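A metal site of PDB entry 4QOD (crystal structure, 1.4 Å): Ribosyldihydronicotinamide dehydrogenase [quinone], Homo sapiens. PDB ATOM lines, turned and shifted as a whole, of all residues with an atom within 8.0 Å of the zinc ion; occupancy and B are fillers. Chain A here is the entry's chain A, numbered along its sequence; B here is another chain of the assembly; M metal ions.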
ATOM      1  N   TYR A 133      19.273  -0.067   6.139  1.00  0.00           N
ATOM      2  CA  TYR A 133      20.075   0.748   7.043  1.00  0.00           C
ATOM      3  C   TYR A 133      20.228   0.003   8.379  1.00  0.00           C
ATOM      4  O   TYR A 133      20.623  -1.099   8.363  1.00  0.00           O
ATOM      5  CB  TYR A 133      19.607   2.229   7.144  1.00  0.00           C
ATOM      6  CG  TYR A 133      19.895   3.021   5.857  1.00  0.00           C
ATOM      7  CD1 TYR A 133      21.187   3.217   5.423  1.00  0.00           C
ATOM      8  CD2 TYR A 133      18.879   3.557   5.115  1.00  0.00           C
ATOM      9  CE1 TYR A 133      21.465   3.912   4.271  1.00  0.00           C
ATOM     10  CE2 TYR A 133      19.136   4.245   3.943  1.00  0.00           C
ATOM     11  CZ  TYR A 133      20.430   4.425   3.536  1.00  0.00           C
ATOM     12  OH  TYR A 133      20.692   5.105   2.396  1.00  0.00           O
ATOM     13  N   ASP A 134      19.871   0.595   9.505  1.00  0.00           N
ATOM     14  CA  ASP A 134      20.089  -0.071  10.798  1.00  0.00           C
ATOM     15  C   ASP A 134      19.337  -1.416  10.931  1.00  0.00           C
ATOM     16  O   ASP A 134      19.710  -2.216  11.718  1.00  0.00           O
ATOM     17  CB  ASP A 134      19.780   0.855  11.957  1.00  0.00           C
ATOM     18  CG  ASP A 134      20.753   1.986  12.092  1.00  0.00           C
ATOM     19  OD1 ASP A 134      21.814   1.982  11.503  1.00  0.00           O
ATOM     20  OD2 ASP A 134      20.411   2.890  12.847  1.00  0.00           O
ATOM     21  N   TRP A 170      30.777   8.124   0.599  1.00  0.00           N
ATOM     22  CA  TRP A 170      29.400   8.065   0.908  1.00  0.00           C
ATOM     23  C   TRP A 170      28.612   6.962   0.154  1.00  0.00           C
ATOM     24  O   TRP A 170      27.861   6.235   0.810  1.00  0.00           O
ATOM     25  CB  TRP A 170      28.763   9.495   0.691  1.00  0.00           C
ATOM     26  CG  TRP A 170      27.302   9.600   0.787  1.00  0.00           C
ATOM     27  CD1 TRP A 170      26.378   9.884  -0.250  1.00  0.00           C
ATOM     28  CD2 TRP A 170      26.544   9.659   1.982  1.00  0.00           C
ATOM     29  NE1 TRP A 170      25.126  10.016   0.271  1.00  0.00           N
ATOM     30  CE2 TRP A 170      25.203   9.973   1.639  1.00  0.00           C
ATOM     31  CE3 TRP A 170      26.885   9.570   3.345  1.00  0.00           C
ATOM     32  CZ2 TRP A 170      24.181  10.060   2.603  1.00  0.00           C
ATOM     33  CZ3 TRP A 170      25.875   9.656   4.264  1.00  0.00           C
ATOM     34  CH2 TRP A 170      24.558   9.974   3.926  1.00  0.00           C
ATOM     35  N   LEU A 172      29.524   4.200  -1.009  1.00  0.00           N
ATOM     36  CA  LEU A 172      30.065   2.910  -0.585  1.00  0.00           C
ATOM     37  C   LEU A 172      29.745   2.576   0.858  1.00  0.00           C
ATOM     38  O   LEU A 172      29.091   1.581   1.181  1.00  0.00           O
ATOM     39  CB  LEU A 172      31.563   2.859  -0.832  1.00  0.00           C
ATOM     40  CG  LEU A 172      32.054   3.051  -2.299  1.00  0.00           C
ATOM     41  CD1 LEU A 172      33.565   3.180  -2.457  1.00  0.00           C
ATOM     42  CD2 LEU A 172      31.578   1.904  -3.145  1.00  0.00           C
ATOM     43  N   GLN A 173      30.223   3.423   1.734  1.00  0.00           N
ATOM     44  CA  GLN A 173      29.950   3.246   3.170  1.00  0.00           C
ATOM     45  C   GLN A 173      28.456   3.315   3.570  1.00  0.00           C
ATOM     46  O   GLN A 173      28.007   2.424   4.268  1.00  0.00           O
ATOM     47  CB  GLN A 173      30.824   4.224   4.006  1.00  0.00           C
ATOM     48  CG  GLN A 173      32.259   3.986   3.845  1.00  0.00           C
ATOM     49  CD  GLN A 173      33.182   4.712   4.838  1.00  0.00           C
ATOM     50  OE1 GLN A 173      34.330   4.293   5.113  1.00  0.00           O
ATOM     51  NE2 GLN A 173      32.749   5.888   5.275  1.00  0.00           N
ATOM     52  N   HIS A 174      27.794   4.363   3.106  1.00  0.00           N
ATOM     53  CA  HIS A 174      26.440   4.576   3.484  1.00  0.00           C
ATOM     54  C   HIS A 174      25.428   3.925   2.520  1.00  0.00           C
ATOM     55  O   HIS A 174      24.620   3.139   2.931  1.00  0.00           O
ATOM     56  CB  HIS A 174      26.185   6.097   3.573  1.00  0.00           C
ATOM     57  CG  HIS A 174      24.824   6.412   4.063  1.00  0.00           C
ATOM     58  ND1 HIS A 174      24.426   6.207   5.371  1.00  0.00           N
ATOM     59  CD2 HIS A 174      23.714   6.833   3.419  1.00  0.00           C
ATOM     60  CE1 HIS A 174      23.183   6.601   5.530  1.00  0.00           C
ATOM     61  NE2 HIS A 174      22.721   6.931   4.350  1.00  0.00           N
ATOM     62  N   GLY A 175      25.499   4.307   1.258  1.00  0.00           N
ATOM     63  CA  GLY A 175      24.547   3.809   0.291  1.00  0.00           C
ATOM     64  C   GLY A 175      24.565   2.299   0.051  1.00  0.00           C
ATOM     65  O   GLY A 175      23.545   1.801  -0.374  1.00  0.00           O
ATOM     66  N   THR A 176      25.724   1.674   0.312  1.00  0.00           N
ATOM     67  CA  THR A 176      25.851   0.220   0.096  1.00  0.00           C
ATOM     68  C   THR A 176      26.017  -0.508   1.438  1.00  0.00           C
ATOM     69  O   THR A 176      25.066  -1.249   1.805  1.00  0.00           O
ATOM     70  CB  THR A 176      27.036  -0.065  -0.769  1.00  0.00           C
ATOM     71  OG1 THR A 176      26.948   0.706  -1.990  1.00  0.00           O
ATOM     72  CG2 THR A 176      27.000  -1.538  -1.217  1.00  0.00           C
ATOM     73  N   LEU A 177      27.018  -0.250   2.231  1.00  0.00           N
ATOM     74  CA  LEU A 177      27.310  -1.120   3.337  1.00  0.00           C
ATOM     75  C   LEU A 177      26.303  -0.861   4.488  1.00  0.00           C
ATOM     76  O   LEU A 177      25.730  -1.789   5.013  1.00  0.00           O
ATOM     77  CB  LEU A 177      28.773  -0.969   3.740  1.00  0.00           C
ATOM     78  CG  LEU A 177      29.813  -1.387   2.672  1.00  0.00           C
ATOM     79  CD1 LEU A 177      31.215  -0.907   3.015  1.00  0.00           C
ATOM     80  CD2 LEU A 177      29.767  -2.846   2.369  1.00  0.00           C
ATOM     81  N   HIS A 178      26.188   0.395   4.903  1.00  0.00           N
ATOM     82  CA  HIS A 178      25.236   0.717   5.940  1.00  0.00           C
ATOM     83  C   HIS A 178      23.810   0.329   5.528  1.00  0.00           C
ATOM     84  O   HIS A 178      23.004  -0.202   6.293  1.00  0.00           O
ATOM     85  CB  HIS A 178      25.325   2.203   6.241  1.00  0.00           C
ATOM     86  CG  HIS A 178      24.511   2.637   7.417  1.00  0.00           C
ATOM     87  ND1 HIS A 178      24.452   3.950   7.791  1.00  0.00           N
ATOM     88  CD2 HIS A 178      23.727   1.971   8.289  1.00  0.00           C
ATOM     89  CE1 HIS A 178      23.658   4.110   8.823  1.00  0.00           C
ATOM     90  NE2 HIS A 178      23.203   2.925   9.154  1.00  0.00           N
ATOM     91  N   PHE A 179      23.474   0.542   4.232  1.00  0.00           N
ATOM     92  CA  PHE A 179      22.204   0.148   3.726  1.00  0.00           C
ATOM     93  C   PHE A 179      21.903  -1.320   4.038  1.00  0.00           C
ATOM     94  O   PHE A 179      20.738  -1.675   4.329  1.00  0.00           O
ATOM     95  CB  PHE A 179      22.035   0.472   2.229  1.00  0.00           C
ATOM     96  CG  PHE A 179      20.676   0.290   1.715  1.00  0.00           C
ATOM     97  CD1 PHE A 179      20.220  -0.903   1.193  1.00  0.00           C
ATOM     98  CD2 PHE A 179      19.824   1.342   1.673  1.00  0.00           C
ATOM     99  CE1 PHE A 179      18.964  -1.060   0.737  1.00  0.00           C
ATOM    100  CE2 PHE A 179      18.531   1.191   1.161  1.00  0.00           C
ATOM    101  CZ  PHE A 179      18.124  -0.009   0.649  1.00  0.00           C
ATOM    102  N   PHE A 182      25.571  -3.313   7.682  1.00  0.00           N
ATOM    103  CA  PHE A 182      26.879  -3.341   8.236  1.00  0.00           C
ATOM    104  C   PHE A 182      27.146  -2.131   9.136  1.00  0.00           C
ATOM    105  O   PHE A 182      26.654  -1.044   8.824  1.00  0.00           O
ATOM    106  CB  PHE A 182      27.960  -3.255   7.151  1.00  0.00           C
ATOM    107  CG  PHE A 182      28.202  -4.495   6.346  1.00  0.00           C
ATOM    108  CD1 PHE A 182      29.107  -5.494   6.790  1.00  0.00           C
ATOM    109  CD2 PHE A 182      27.683  -4.576   5.085  1.00  0.00           C
ATOM    110  CE1 PHE A 182      29.306  -6.614   5.997  1.00  0.00           C
ATOM    111  CE2 PHE A 182      27.887  -5.712   4.278  1.00  0.00           C
ATOM    112  CZ  PHE A 182      28.759  -6.695   4.748  1.00  0.00           C
ATOM    113  N   VAL A 184      30.383   0.091   9.945  1.00  0.00           N
ATOM    114  CA  VAL A 184      31.470   0.468   9.108  1.00  0.00           C
ATOM    115  C   VAL A 184      32.648   0.931   9.966  1.00  0.00           C
ATOM    116  O   VAL A 184      32.572   1.898  10.752  1.00  0.00           O
ATOM    117  CB  VAL A 184      31.057   1.571   8.116  1.00  0.00           C
ATOM    118  CG1 VAL A 184      32.238   2.087   7.327  1.00  0.00           C
ATOM    119  CG2 VAL A 184      29.905   1.132   7.247  1.00  0.00           C
ATOM    120  N   ILE A 221      32.454   3.832  12.868  1.00  0.00           N
ATOM    121  CA  ILE A 221      32.091   5.211  12.691  1.00  0.00           C
ATOM    122  C   ILE A 221      30.570   5.411  12.829  1.00  0.00           C
ATOM    123  O   ILE A 221      29.709   4.493  12.666  1.00  0.00           O
ATOM    124  CB  ILE A 221      32.596   5.739  11.328  1.00  0.00           C
ATOM    125  CG1 ILE A 221      31.806   5.085  10.175  1.00  0.00           C
ATOM    126  CG2 ILE A 221      34.100   5.582  11.202  1.00  0.00           C
ATOM    127  CD1 ILE A 221      31.998   5.774   8.840  1.00  0.00           C
ATOM    128  N   PRO A 222      30.185   6.674  13.093  1.00  0.00           N
ATOM    129  CA  PRO A 222      28.805   7.040  12.883  1.00  0.00           C
ATOM    130  C   PRO A 222      28.576   7.339  11.372  1.00  0.00           C
ATOM    131  O   PRO A 222      29.071   8.328  10.875  1.00  0.00           O
ATOM    132  CB  PRO A 222      28.655   8.341  13.749  1.00  0.00           C
ATOM    133  CG  PRO A 222      30.073   8.965  13.687  1.00  0.00           C
ATOM    134  CD  PRO A 222      31.014   7.801  13.582  1.00  0.00           C
ATOM    135  N   CYS A 223      27.938   6.372  10.689  1.00  0.00           N
ATOM    136  CA  CYS A 223      27.889   6.409   9.238  1.00  0.00           C
ATOM    137  C   CYS A 223      26.661   7.277   8.824  1.00  0.00           C
ATOM    138  O   CYS A 223      25.637   6.809   8.369  1.00  0.00           O
ATOM    139  CB  CYS A 223      27.798   4.981   8.651  1.00  0.00           C
ATOM    140  SG  CYS A 223      27.770   5.005   6.842  1.00  0.00           S
ATOM    141  N   THR A 224      26.870   8.578   8.967  1.00  0.00           N
ATOM    142  CA  THR A 224      25.848   9.602   8.794  1.00  0.00           C
ATOM    143  C   THR A 224      26.364  10.647   7.777  1.00  0.00           C
ATOM    144  O   THR A 224      27.543  10.805   7.476  1.00  0.00           O
ATOM    145  CB  THR A 224      25.644  10.316  10.161  1.00  0.00           C
ATOM    146  OG1 THR A 224      26.828  10.997  10.527  1.00  0.00           O
ATOM    147  CG2 THR A 224      25.186   9.340  11.262  1.00  0.00           C
ATOM    148  N   ALA A 225      25.380  11.417   7.334  1.00  0.00           N
ATOM    149  CA  ALA A 225      25.683  12.555   6.485  1.00  0.00           C
ATOM    150  C   ALA A 225      26.666  13.535   7.151  1.00  0.00           C
ATOM    151  O   ALA A 225      27.663  14.006   6.578  1.00  0.00           O
ATOM    152  CB  ALA A 225      24.420  13.254   6.052  1.00  0.00           C
ATOM    153  N   TRP A 227      29.009  12.891   9.427  1.00  0.00           N
ATOM    154  CA  TRP A 227      30.346  12.372   9.345  1.00  0.00           C
ATOM    155  C   TRP A 227      31.033  12.559   8.014  1.00  0.00           C
ATOM    156  O   TRP A 227      32.192  12.952   7.947  1.00  0.00           O
ATOM    157  CB  TRP A 227      30.366  10.861   9.770  1.00  0.00           C
ATOM    158  CG  TRP A 227      31.738  10.274   9.899  1.00  0.00           C
ATOM    159  CD1 TRP A 227      32.484  10.146  11.063  1.00  0.00           C
ATOM    160  CD2 TRP A 227      32.542   9.660   8.878  1.00  0.00           C
ATOM    161  NE1 TRP A 227      33.688   9.534  10.828  1.00  0.00           N
ATOM    162  CE2 TRP A 227      33.720   9.180   9.475  1.00  0.00           C
ATOM    163  CE3 TRP A 227      32.349   9.431   7.500  1.00  0.00           C
ATOM    164  CZ2 TRP A 227      34.764   8.586   8.756  1.00  0.00           C
ATOM    165  CZ3 TRP A 227      33.431   8.867   6.795  1.00  0.00           C
ATOM    166  CH2 TRP A 227      34.593   8.440   7.409  1.00  0.00           C
ATOM    167  N   HIS A 228      30.260  12.332   6.908  1.00  0.00           N
ATOM    168  CA  HIS A 228      30.888  12.387   5.606  1.00  0.00           C
ATOM    169  C   HIS A 228      31.080  13.833   5.086  1.00  0.00           C
ATOM    170  O   HIS A 228      32.100  14.101   4.429  1.00  0.00           O
ATOM    171  CB  HIS A 228      30.004  11.610   4.625  1.00  0.00           C
ATOM    172  CG  HIS A 228      30.074  10.123   4.780  1.00  0.00           C
ATOM    173  ND1 HIS A 228      29.315   9.423   5.681  1.00  0.00           N
ATOM    174  CD2 HIS A 228      30.824   9.214   4.095  1.00  0.00           C
ATOM    175  CE1 HIS A 228      29.600   8.114   5.579  1.00  0.00           C
ATOM    176  NE2 HIS A 228      30.536   7.964   4.639  1.00  0.00           N
ATOM    177  N   VAL B 161      16.590   9.613   4.520  1.00  0.00           N
ATOM    178  CA  VAL B 161      17.565   8.443   4.865  1.00  0.00           C
ATOM    179  C   VAL B 161      18.791   8.258   3.930  1.00  0.00           C
ATOM    180  O   VAL B 161      19.963   7.868   4.330  1.00  0.00           O
ATOM    181  CB  VAL B 161      16.820   7.093   5.109  1.00  0.00           C
ATOM    182  CG1 VAL B 161      15.979   7.228   6.369  1.00  0.00           C
ATOM    183  CG2 VAL B 161      15.919   6.611   3.945  1.00  0.00           C
HETATM  184 ZN    ZN M   1      25.582   5.440   6.918  1.00  0.00          ZN
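Thr 224 touches the zinc ion. Within 4 Å of the zinc ion: His 174, His 178, Cys 223 and Thr 224. The nearest printed residue that does not touch the zinc ion is Gln 173 (4.7 Å).
The zinc ion is bound by the backbone carbonyl oxygen of Cys 223, a ring nitrogen (ND1) of His 178, a ring nitrogen (ND1) of His 174 and the side-chain sulfur of Cys 223.
The backbone carbonyl oxygen of Gln 173 lies close to the side-chain sulfur of Cys 223 (3.7 Å). O of Gln 173 sits at hydrogen-bond distance from N of His 178, at 2.8 Å. OD1 of Asp 134 lies within hydrogen-bond range of NE2 of His 178 (2.9 Å). The side-chain hydroxyl (OH) of Tyr 133 lies close to a ring nitrogen (NE2) of His 174. The backbone carbonyl oxygen (O) of His 174 lies within hydrogen-bond range of the backbone NH (N) of Phe 179 (3.1 Å). A ring nitrogen (NE2) of His 174 lies within hydrogen-bond range of the backbone carbonyl oxygen of Val 161 of chain B (2.9 Å). A ring nitrogen (ND1) of His 228 sits at hydrogen-bond distance from the backbone carbonyl oxygen of Thr 224 (2.9 Å). OG1 of Thr 224 sits at hydrogen-bond distance from N of Trp 227 (3.1 Å).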
